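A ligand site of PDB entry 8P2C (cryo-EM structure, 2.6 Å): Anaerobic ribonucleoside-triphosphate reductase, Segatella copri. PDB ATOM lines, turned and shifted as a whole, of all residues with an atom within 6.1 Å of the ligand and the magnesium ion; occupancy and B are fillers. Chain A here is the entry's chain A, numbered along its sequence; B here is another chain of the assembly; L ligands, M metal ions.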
ATOM      1  N   PHE A 188       1.561   9.903 -27.957  1.00  0.00           N
ATOM      2  CA  PHE A 188       1.834  11.326 -28.015  1.00  0.00           C
ATOM      3  C   PHE A 188       1.147  12.016 -26.852  1.00  0.00           C
ATOM      4  O   PHE A 188       0.062  11.615 -26.419  1.00  0.00           O
ATOM      5  CB  PHE A 188       1.383  11.955 -29.342  1.00  0.00           C
ATOM      6  CG  PHE A 188      -0.066  11.751 -29.664  1.00  0.00           C
ATOM      7  CD1 PHE A 188      -1.031  12.629 -29.193  1.00  0.00           C
ATOM      8  CD2 PHE A 188      -0.474  10.689 -30.458  1.00  0.00           C
ATOM      9  CE1 PHE A 188      -2.356  12.452 -29.499  1.00  0.00           C
ATOM     10  CE2 PHE A 188      -1.801  10.502 -30.762  1.00  0.00           C
ATOM     11  CZ  PHE A 188      -2.752  11.389 -30.287  1.00  0.00           C
ATOM     12  N   SER A 194      -3.352  12.431 -23.585  1.00  0.00           N
ATOM     13  CA  SER A 194      -2.312  11.464 -23.882  1.00  0.00           C
ATOM     14  C   SER A 194      -2.949  10.255 -24.550  1.00  0.00           C
ATOM     15  O   SER A 194      -4.141   9.982 -24.373  1.00  0.00           O
ATOM     16  CB  SER A 194      -1.544  11.051 -22.631  1.00  0.00           C
ATOM     17  OG  SER A 194      -0.511  10.123 -22.944  1.00  0.00           O
ATOM     18  N   SER A 195      -2.139   9.524 -25.319  1.00  0.00           N
ATOM     19  CA  SER A 195      -2.589   8.335 -26.008  1.00  0.00           C
ATOM     20  C   SER A 195      -1.518   7.263 -25.940  1.00  0.00           C
ATOM     21  O   SER A 195      -0.326   7.566 -25.820  1.00  0.00           O
ATOM     22  CB  SER A 195      -2.948   8.634 -27.472  1.00  0.00           C
ATOM     23  OG  SER A 195      -4.021   9.548 -27.555  1.00  0.00           O
ATOM     24  N   ARG A 196      -1.953   6.014 -26.006  1.00  0.00           N
ATOM     25  CA  ARG A 196      -1.111   4.832 -25.933  1.00  0.00           C
ATOM     26  C   ARG A 196      -0.833   4.281 -27.316  1.00  0.00           C
ATOM     27  O   ARG A 196      -1.518   4.636 -28.286  1.00  0.00           O
ATOM     28  CB  ARG A 196      -1.787   3.761 -25.055  1.00  0.00           C
ATOM     29  CG  ARG A 196      -2.080   4.240 -23.635  1.00  0.00           C
ATOM     30  CD  ARG A 196      -2.544   3.110 -22.740  1.00  0.00           C
ATOM     31  NE  ARG A 196      -3.925   2.702 -23.003  1.00  0.00           N
ATOM     32  CZ  ARG A 196      -4.980   3.150 -22.332  1.00  0.00           C
ATOM     33  NH1 ARG A 196      -4.850   4.013 -21.349  1.00  0.00           N
ATOM     34  NH2 ARG A 196      -6.183   2.695 -22.645  1.00  0.00           N
ATOM     35  N   PRO A 197       0.188   3.429 -27.470  1.00  0.00           N
ATOM     36  CA  PRO A 197       0.488   2.875 -28.796  1.00  0.00           C
ATOM     37  C   PRO A 197      -0.681   2.102 -29.378  1.00  0.00           C
ATOM     38  O   PRO A 197      -1.468   1.466 -28.669  1.00  0.00           O
ATOM     39  CB  PRO A 197       1.678   1.962 -28.523  1.00  0.00           C
ATOM     40  CG  PRO A 197       2.355   2.576 -27.358  1.00  0.00           C
ATOM     41  CD  PRO A 197       1.246   3.121 -26.501  1.00  0.00           C
ATOM     42  N   ALA A 198      -0.804   2.167 -30.707  1.00  0.00           N
ATOM     43  CA  ALA A 198      -1.901   1.525 -31.403  1.00  0.00           C
ATOM     44  C   ALA A 198      -1.750   0.013 -31.378  1.00  0.00           C
ATOM     45  O   ALA A 198      -0.642  -0.529 -31.366  1.00  0.00           O
ATOM     46  CB  ALA A 198      -1.979   2.014 -32.846  1.00  0.00           C
ATOM     47  N   LYS A 199      -2.887  -0.686 -31.374  1.00  0.00           N
ATOM     48  CA  LYS A 199      -2.920  -2.137 -31.384  1.00  0.00           C
ATOM     49  C   LYS A 199      -3.731  -2.726 -32.519  1.00  0.00           C
ATOM     50  O   LYS A 199      -3.763  -3.949 -32.673  1.00  0.00           O
ATOM     51  CB  LYS A 199      -3.459  -2.670 -30.045  1.00  0.00           C
ATOM     52  CG  LYS A 199      -2.844  -2.013 -28.818  1.00  0.00           C
ATOM     53  CD  LYS A 199      -1.365  -2.348 -28.686  1.00  0.00           C
ATOM     54  CE  LYS A 199      -1.163  -3.796 -28.309  1.00  0.00           C
ATOM     55  NZ  LYS A 199      -1.824  -4.136 -27.023  1.00  0.00           N
ATOM     56  N   ARG A 200      -4.393  -1.898 -33.333  1.00  0.00           N
ATOM     57  CA  ARG A 200      -5.259  -2.353 -34.413  1.00  0.00           C
ATOM     58  C   ARG A 200      -5.159  -1.355 -35.559  1.00  0.00           C
ATOM     59  O   ARG A 200      -4.237  -0.530 -35.602  1.00  0.00           O
ATOM     60  CB  ARG A 200      -6.703  -2.524 -33.915  1.00  0.00           C
ATOM     61  CG  ARG A 200      -6.943  -3.721 -33.035  1.00  0.00           C
ATOM     62  CD  ARG A 200      -8.378  -3.755 -32.572  1.00  0.00           C
ATOM     63  NE  ARG A 200      -8.709  -2.591 -31.760  1.00  0.00           N
ATOM     64  CZ  ARG A 200      -8.510  -2.506 -30.455  1.00  0.00           C
ATOM     65  NH1 ARG A 200      -7.974  -3.498 -29.779  1.00  0.00           N
ATOM     66  NH2 ARG A 200      -8.858  -1.386 -29.819  1.00  0.00           N
ATOM     67  N   GLU A 202      -8.227   0.226 -36.532  1.00  0.00           N
ATOM     68  CA  GLU A 202      -9.269   1.180 -36.149  1.00  0.00           C
ATOM     69  C   GLU A 202      -8.731   2.308 -35.294  1.00  0.00           C
ATOM     70  O   GLU A 202      -9.314   3.395 -35.293  1.00  0.00           O
ATOM     71  CB  GLU A 202     -10.396   0.468 -35.402  1.00  0.00           C
ATOM     72  CG  GLU A 202     -11.185  -0.525 -36.234  1.00  0.00           C
ATOM     73  CD  GLU A 202     -10.691  -1.945 -36.063  1.00  0.00           C
ATOM     74  OE1 GLU A 202      -9.574  -2.135 -35.536  1.00  0.00           O
ATOM     75  OE2 GLU A 202     -11.437  -2.881 -36.434  1.00  0.00           O
ATOM     76  N   THR A 203      -7.648   2.074 -34.553  1.00  0.00           N
ATOM     77  CA  THR A 203      -7.016   3.139 -33.786  1.00  0.00           C
ATOM     78  C   THR A 203      -5.879   3.816 -34.550  1.00  0.00           C
ATOM     79  O   THR A 203      -5.642   5.010 -34.341  1.00  0.00           O
ATOM     80  CB  THR A 203      -6.477   2.589 -32.463  1.00  0.00           C
ATOM     81  OG1 THR A 203      -5.589   1.498 -32.721  1.00  0.00           O
ATOM     82  CG2 THR A 203      -7.624   2.111 -31.593  1.00  0.00           C
ATOM     83  N   VAL A 206      -7.435   6.537 -36.778  1.00  0.00           N
ATOM     84  CA  VAL A 206      -7.912   7.667 -35.984  1.00  0.00           C
ATOM     85  C   VAL A 206      -6.736   8.480 -35.453  1.00  0.00           C
ATOM     86  O   VAL A 206      -6.796   9.718 -35.393  1.00  0.00           O
ATOM     87  CB  VAL A 206      -8.825   7.169 -34.847  1.00  0.00           C
ATOM     88  CG1 VAL A 206      -9.233   8.328 -33.961  1.00  0.00           C
ATOM     89  CG2 VAL A 206     -10.049   6.496 -35.432  1.00  0.00           C
ATOM     90  N   LEU A 207      -5.651   7.812 -35.068  1.00  0.00           N
ATOM     91  CA  LEU A 207      -4.472   8.550 -34.598  1.00  0.00           C
ATOM     92  C   LEU A 207      -3.841   9.360 -35.725  1.00  0.00           C
ATOM     93  O   LEU A 207      -3.374  10.482 -35.500  1.00  0.00           O
ATOM     94  CB  LEU A 207      -3.457   7.577 -33.988  1.00  0.00           C
ATOM     95  CG  LEU A 207      -3.465   7.459 -32.459  1.00  0.00           C
ATOM     96  CD1 LEU A 207      -4.842   7.076 -31.943  1.00  0.00           C
ATOM     97  CD2 LEU A 207      -2.432   6.441 -32.003  1.00  0.00           C
ATOM     98  N   ILE A 210      -5.933  12.407 -36.046  1.00  0.00           N
ATOM     99  CA  ILE A 210      -5.692  13.338 -34.955  1.00  0.00           C
ATOM    100  C   ILE A 210      -4.392  14.103 -35.170  1.00  0.00           C
ATOM    101  O   ILE A 210      -4.323  15.308 -34.929  1.00  0.00           O
ATOM    102  CB  ILE A 210      -5.715  12.598 -33.601  1.00  0.00           C
ATOM    103  CG1 ILE A 210      -7.160  12.410 -33.142  1.00  0.00           C
ATOM    104  CG2 ILE A 210      -4.903  13.354 -32.557  1.00  0.00           C
ATOM    105  CD1 ILE A 210      -7.303  12.198 -31.666  1.00  0.00           C
ATOM    106  N   ASN B 290     -16.841  -6.123 -25.506  1.00  0.00           N
ATOM    107  CA  ASN B 290     -15.531  -5.599 -25.882  1.00  0.00           C
ATOM    108  C   ASN B 290     -15.666  -4.415 -26.841  1.00  0.00           C
ATOM    109  O   ASN B 290     -14.984  -3.390 -26.687  1.00  0.00           O
ATOM    110  CB  ASN B 290     -14.688  -6.699 -26.514  1.00  0.00           C
ATOM    111  CG  ASN B 290     -13.380  -6.181 -27.077  1.00  0.00           C
ATOM    112  OD1 ASN B 290     -13.308  -5.791 -28.239  1.00  0.00           O
ATOM    113  ND2 ASN B 290     -12.347  -6.176 -26.258  1.00  0.00           N
ATOM    114  N   HIS B 293     -16.952  -1.327 -25.033  1.00  0.00           N
ATOM    115  CA  HIS B 293     -15.876  -0.806 -24.186  1.00  0.00           C
ATOM    116  C   HIS B 293     -14.897   0.028 -24.999  1.00  0.00           C
ATOM    117  O   HIS B 293     -14.550   1.158 -24.619  1.00  0.00           O
ATOM    118  CB  HIS B 293     -15.165  -1.978 -23.505  1.00  0.00           C
ATOM    119  CG  HIS B 293     -13.928  -1.584 -22.762  1.00  0.00           C
ATOM    120  ND1 HIS B 293     -13.958  -0.811 -21.628  1.00  0.00           N
ATOM    121  CD2 HIS B 293     -12.627  -1.892 -22.976  1.00  0.00           C
ATOM    122  CE1 HIS B 293     -12.726  -0.632 -21.183  1.00  0.00           C
ATOM    123  NE2 HIS B 293     -11.896  -1.279 -21.981  1.00  0.00           N
ATOM    124  N   GLN B 294     -14.446  -0.509 -26.136  1.00  0.00           N
ATOM    125  CA  GLN B 294     -13.514   0.232 -26.983  1.00  0.00           C
ATOM    126  C   GLN B 294     -14.146   1.517 -27.505  1.00  0.00           C
ATOM    127  O   GLN B 294     -13.478   2.561 -27.570  1.00  0.00           O
ATOM    128  CB  GLN B 294     -13.037  -0.642 -28.134  1.00  0.00           C
ATOM    129  CG  GLN B 294     -12.315  -1.905 -27.692  1.00  0.00           C
ATOM    130  CD  GLN B 294     -10.922  -1.649 -27.155  1.00  0.00           C
ATOM    131  OE1 GLN B 294      -9.938  -1.808 -27.876  1.00  0.00           O
ATOM    132  NE2 GLN B 294     -10.832  -1.269 -25.892  1.00  0.00           N
ATOM    133  N   GLU B 297     -14.193   4.121 -24.704  1.00  0.00           N
ATOM    134  CA  GLU B 297     -12.828   4.587 -24.467  1.00  0.00           C
ATOM    135  C   GLU B 297     -12.389   5.581 -25.543  1.00  0.00           C
ATOM    136  O   GLU B 297     -11.784   6.618 -25.235  1.00  0.00           O
ATOM    137  CB  GLU B 297     -11.870   3.393 -24.423  1.00  0.00           C
ATOM    138  CG  GLU B 297     -10.440   3.739 -24.078  1.00  0.00           C
ATOM    139  CD  GLU B 297      -9.532   2.528 -24.101  1.00  0.00           C
ATOM    140  OE1 GLU B 297      -9.869   1.548 -24.792  1.00  0.00           O
ATOM    141  OE2 GLU B 297      -8.494   2.548 -23.411  1.00  0.00           O
ATOM    142  N   ALA B 298     -12.714   5.278 -26.800  1.00  0.00           N
ATOM    143  CA  ALA B 298     -12.387   6.193 -27.886  1.00  0.00           C
ATOM    144  C   ALA B 298     -13.125   7.530 -27.729  1.00  0.00           C
ATOM    145  O   ALA B 298     -12.550   8.590 -27.982  1.00  0.00           O
ATOM    146  CB  ALA B 298     -12.732   5.555 -29.228  1.00  0.00           C
ATOM    147  N   PHE B 299     -14.388   7.480 -27.319  1.00  0.00           N
ATOM    148  CA  PHE B 299     -15.139   8.721 -27.090  1.00  0.00           C
ATOM    149  C   PHE B 299     -14.451   9.587 -26.042  1.00  0.00           C
ATOM    150  O   PHE B 299     -14.281  10.801 -26.237  1.00  0.00           O
ATOM    151  CB  PHE B 299     -16.566   8.381 -26.651  1.00  0.00           C
ATOM    152  CG  PHE B 299     -17.435   9.590 -26.408  1.00  0.00           C
ATOM    153  CD1 PHE B 299     -17.440  10.224 -25.183  1.00  0.00           C
ATOM    154  CD2 PHE B 299     -18.255  10.075 -27.396  1.00  0.00           C
ATOM    155  CE1 PHE B 299     -18.238  11.328 -24.951  1.00  0.00           C
ATOM    156  CE2 PHE B 299     -19.058  11.176 -27.182  1.00  0.00           C
ATOM    157  CZ  PHE B 299     -19.043  11.798 -25.950  1.00  0.00           C
ATOM    158  N   HIS B 301     -11.290   9.550 -24.964  1.00  0.00           N
ATOM    159  CA  HIS B 301     -10.006  10.049 -25.434  1.00  0.00           C
ATOM    160  C   HIS B 301     -10.175  11.176 -26.447  1.00  0.00           C
ATOM    161  O   HIS B 301      -9.466  12.186 -26.392  1.00  0.00           O
ATOM    162  CB  HIS B 301      -9.183   8.918 -26.034  1.00  0.00           C
ATOM    163  CG  HIS B 301      -8.467   8.081 -25.023  1.00  0.00           C
ATOM    164  ND1 HIS B 301      -9.114   7.477 -23.959  1.00  0.00           N
ATOM    165  CD2 HIS B 301      -7.161   7.738 -24.908  1.00  0.00           C
ATOM    166  CE1 HIS B 301      -8.235   6.805 -23.238  1.00  0.00           C
ATOM    167  NE2 HIS B 301      -7.049   6.950 -23.790  1.00  0.00           N
ATOM    168  N   ASN B 302     -11.117  11.019 -27.379  1.00  0.00           N
ATOM    169  CA  ASN B 302     -11.377  12.064 -28.355  1.00  0.00           C
ATOM    170  C   ASN B 302     -11.761  13.366 -27.667  1.00  0.00           C
ATOM    171  O   ASN B 302     -11.002  14.334 -27.680  1.00  0.00           O
ATOM    172  CB  ASN B 302     -12.466  11.622 -29.327  1.00  0.00           C
ATOM    173  CG  ASN B 302     -12.655  12.590 -30.476  1.00  0.00           C
ATOM    174  OD1 ASN B 302     -11.960  12.509 -31.480  1.00  0.00           O
ATOM    175  ND2 ASN B 302     -13.604  13.502 -30.329  1.00  0.00           N
ATOM    176  N   THR B 305      -8.848  15.039 -25.972  1.00  0.00           N
ATOM    177  CA  THR B 305      -7.795  15.623 -26.793  1.00  0.00           C
ATOM    178  C   THR B 305      -8.297  16.831 -27.598  1.00  0.00           C
ATOM    179  O   THR B 305      -7.527  17.760 -27.848  1.00  0.00           O
ATOM    180  CB  THR B 305      -7.212  14.578 -27.744  1.00  0.00           C
ATOM    181  OG1 THR B 305      -8.256  14.002 -28.538  1.00  0.00           O
ATOM    182  CG2 THR B 305      -6.505  13.480 -26.959  1.00  0.00           C
ATOM    183  N   GLY B 345      -4.691   7.543 -21.226  1.00  0.00           N
ATOM    184  CA  GLY B 345      -3.273   7.273 -21.372  1.00  0.00           C
ATOM    185  C   GLY B 345      -2.727   6.326 -20.320  1.00  0.00           C
ATOM    186  O   GLY B 345      -3.161   5.170 -20.233  1.00  0.00           O
HETATM  187  P1  LIG L   1      -6.755  -2.460 -25.308  1.00  0.00           P
HETATM  188  O1  LIG L   1      -6.131  -3.636 -25.965  1.00  0.00           O
HETATM  189  O2  LIG L   1      -6.457  -2.352 -23.813  1.00  0.00           O
HETATM  190  O3  LIG L   1      -8.273  -2.360 -25.506  1.00  0.00           O
HETATM  191  P2  LIG L   1      -4.953  -0.116 -25.761  1.00  0.00           P
HETATM  192  O4  LIG L   1      -3.707  -0.834 -25.452  1.00  0.00           O
HETATM  193  O5  LIG L   1      -5.374   0.955 -24.763  1.00  0.00           O
HETATM  194  O6  LIG L   1      -6.184  -1.103 -25.925  1.00  0.00           O
HETATM  195  P3  LIG L   1      -5.859   0.777 -28.438  1.00  0.00           P
HETATM  196  O7  LIG L   1      -5.370   0.069 -29.629  1.00  0.00           O
HETATM  197  O8  LIG L   1      -7.271   0.397 -27.986  1.00  0.00           O
HETATM  198  O9  LIG L   1      -4.887   0.569 -27.201  1.00  0.00           O
HETATM  199  O10 LIG L   1      -5.817   2.351 -28.628  1.00  0.00           O
HETATM  200  C1  LIG L   1      -4.556   3.060 -28.645  1.00  0.00           C
HETATM  201  C2  LIG L   1      -4.711   4.375 -27.924  1.00  0.00           C
HETATM  202  O11 LIG L   1      -5.498   5.287 -28.720  1.00  0.00           O
HETATM  203  C3  LIG L   1      -5.395   4.294 -26.550  1.00  0.00           C
HETATM  204  O12 LIG L   1      -4.664   5.054 -25.590  1.00  0.00           O
HETATM  205  C4  LIG L   1      -6.760   4.927 -26.804  1.00  0.00           C
HETATM  206  C5  LIG L   1      -6.450   5.926 -27.899  1.00  0.00           C
HETATM  207  N1  LIG L   1      -7.584   6.316 -28.716  1.00  0.00           N
HETATM  208  C6  LIG L   1      -8.544   5.500 -29.261  1.00  0.00           C
HETATM  209  N2  LIG L   1      -9.456   6.141 -29.958  1.00  0.00           N
HETATM  210  C7  LIG L   1      -9.072   7.466 -29.861  1.00  0.00           C
HETATM  211  C8  LIG L   1      -9.624   8.660 -30.367  1.00  0.00           C
HETATM  212  N3  LIG L   1     -10.738   8.700 -31.120  1.00  0.00           N
HETATM  213  N4  LIG L   1      -9.000   9.815 -30.073  1.00  0.00           N
HETATM  214  C9  LIG L   1      -7.898   9.775 -29.327  1.00  0.00           C
HETATM  215  N5  LIG L   1      -7.280   8.722 -28.789  1.00  0.00           N
HETATM  216  C10 LIG L   1      -7.924   7.589 -29.091  1.00  0.00           C
HETATM  217 MG    MG M   1      -7.874   0.027 -26.103  1.00  0.00          MG
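O3 of the ligand lies close to NE2 of Gln 294 of chain B.
N of Arg 196 sits at hydrogen-bond distance from O12 of the ligand (2.9 Å).
NH2 of Arg 196 lies within salt-bridge range of O5 of the ligand (2.9 Å).
An oxygen (O7) of the ligand lies within salt-bridge range of the guanidinium group of Arg 200, 3.8 Å away.
An oxygen (O7) of the ligand sits at hydrogen-bond distance from the backbone NH (N) of Lys 199 (3.1 Å).
The side-chain hydroxyl of Thr 203 is in hydrogen-bond range of an oxygen (O7) of the ligand (3.4 Å).
The side-chain carboxylate of Glu 297 of chain B sits at hydrogen-bond distance from the side-chain amide nitrogen of Gln 294 of chain B, at 3.2 Å.
The guanidinium group of Arg 200 lies close to the side-chain amide oxygen of Gln 294 of chain B (3.2 Å).
The side-chain carboxylate of Glu 297 of chain B is in salt-bridge range of the guanidinium group of Arg 196 (2.4 Å).
O of Glu 297 of chain B is in hydrogen-bond range of ND1 of His 301 of chain B (3.1 Å).
The guanidinium group (NE) of Arg 200 lies within salt-bridge range of the side-chain carboxylate (OE1) of Glu 202 (3.9 Å).
O of His 301 of chain B sits at hydrogen-bond distance from OG1 of Thr 305 of chain B (3.1 Å).
The backbone NH (N) of Ser 195 is in hydrogen-bond range of the backbone carbonyl oxygen (O) of Phe 188, at 3.2 Å.
The side-chain hydroxyl (OG1) of Thr 305 of chain B sits at hydrogen-bond distance from the backbone carbonyl oxygen (O) of Asn 302 of chain B.
Ser 195 touches the ligand (OG to N5, 3.6 Å).
Pro 197 touches the ligand.
CG1 of Val 206 touches N3 of the ligand, 3.2 Å away.
CD1 of Leu 207 touches O11 of the ligand (3.7 Å).
CD1 of Ile 210 touches N4 of the ligand, 3.3 Å away.
CB of Ala 298 of chain B touches N2 of the ligand, 3.4 Å away.
His 301 of chain B touches the ligand.
Asn 302 of chain B touches the ligand.
Within 4 Å of the ligand: Ser 195, Arg 196, Pro 197, Lys 199, Arg 200, Thr 203, Val 206, Leu 207, Ile 210, Gln 294 of chain B, Glu 297 of chain B, Ala 298 of chain B, His 301 of chain B and Asn 302 of chain B.
The nearest printed residue that does not touch the ligand is Ala 198 (4.02 Å).
Merely in contact with the magnesium ion: Gln 294 of chain B.
Of the 23 residues printed, 2 come within 4 Å of the magnesium ion.
The nearest printed residue that does not touch the magnesium ion is Arg 200 (4.1 Å).
The magnesium ion is bound by O8 of the ligand (2.0 Å), O6 of the ligand (2.0 Å) and O3 of the ligand (2.5 Å).
Slightly farther from the magnesium ion lies the side-chain carboxylate (OE1) of Glu 297 of chain B (2.8 Å).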
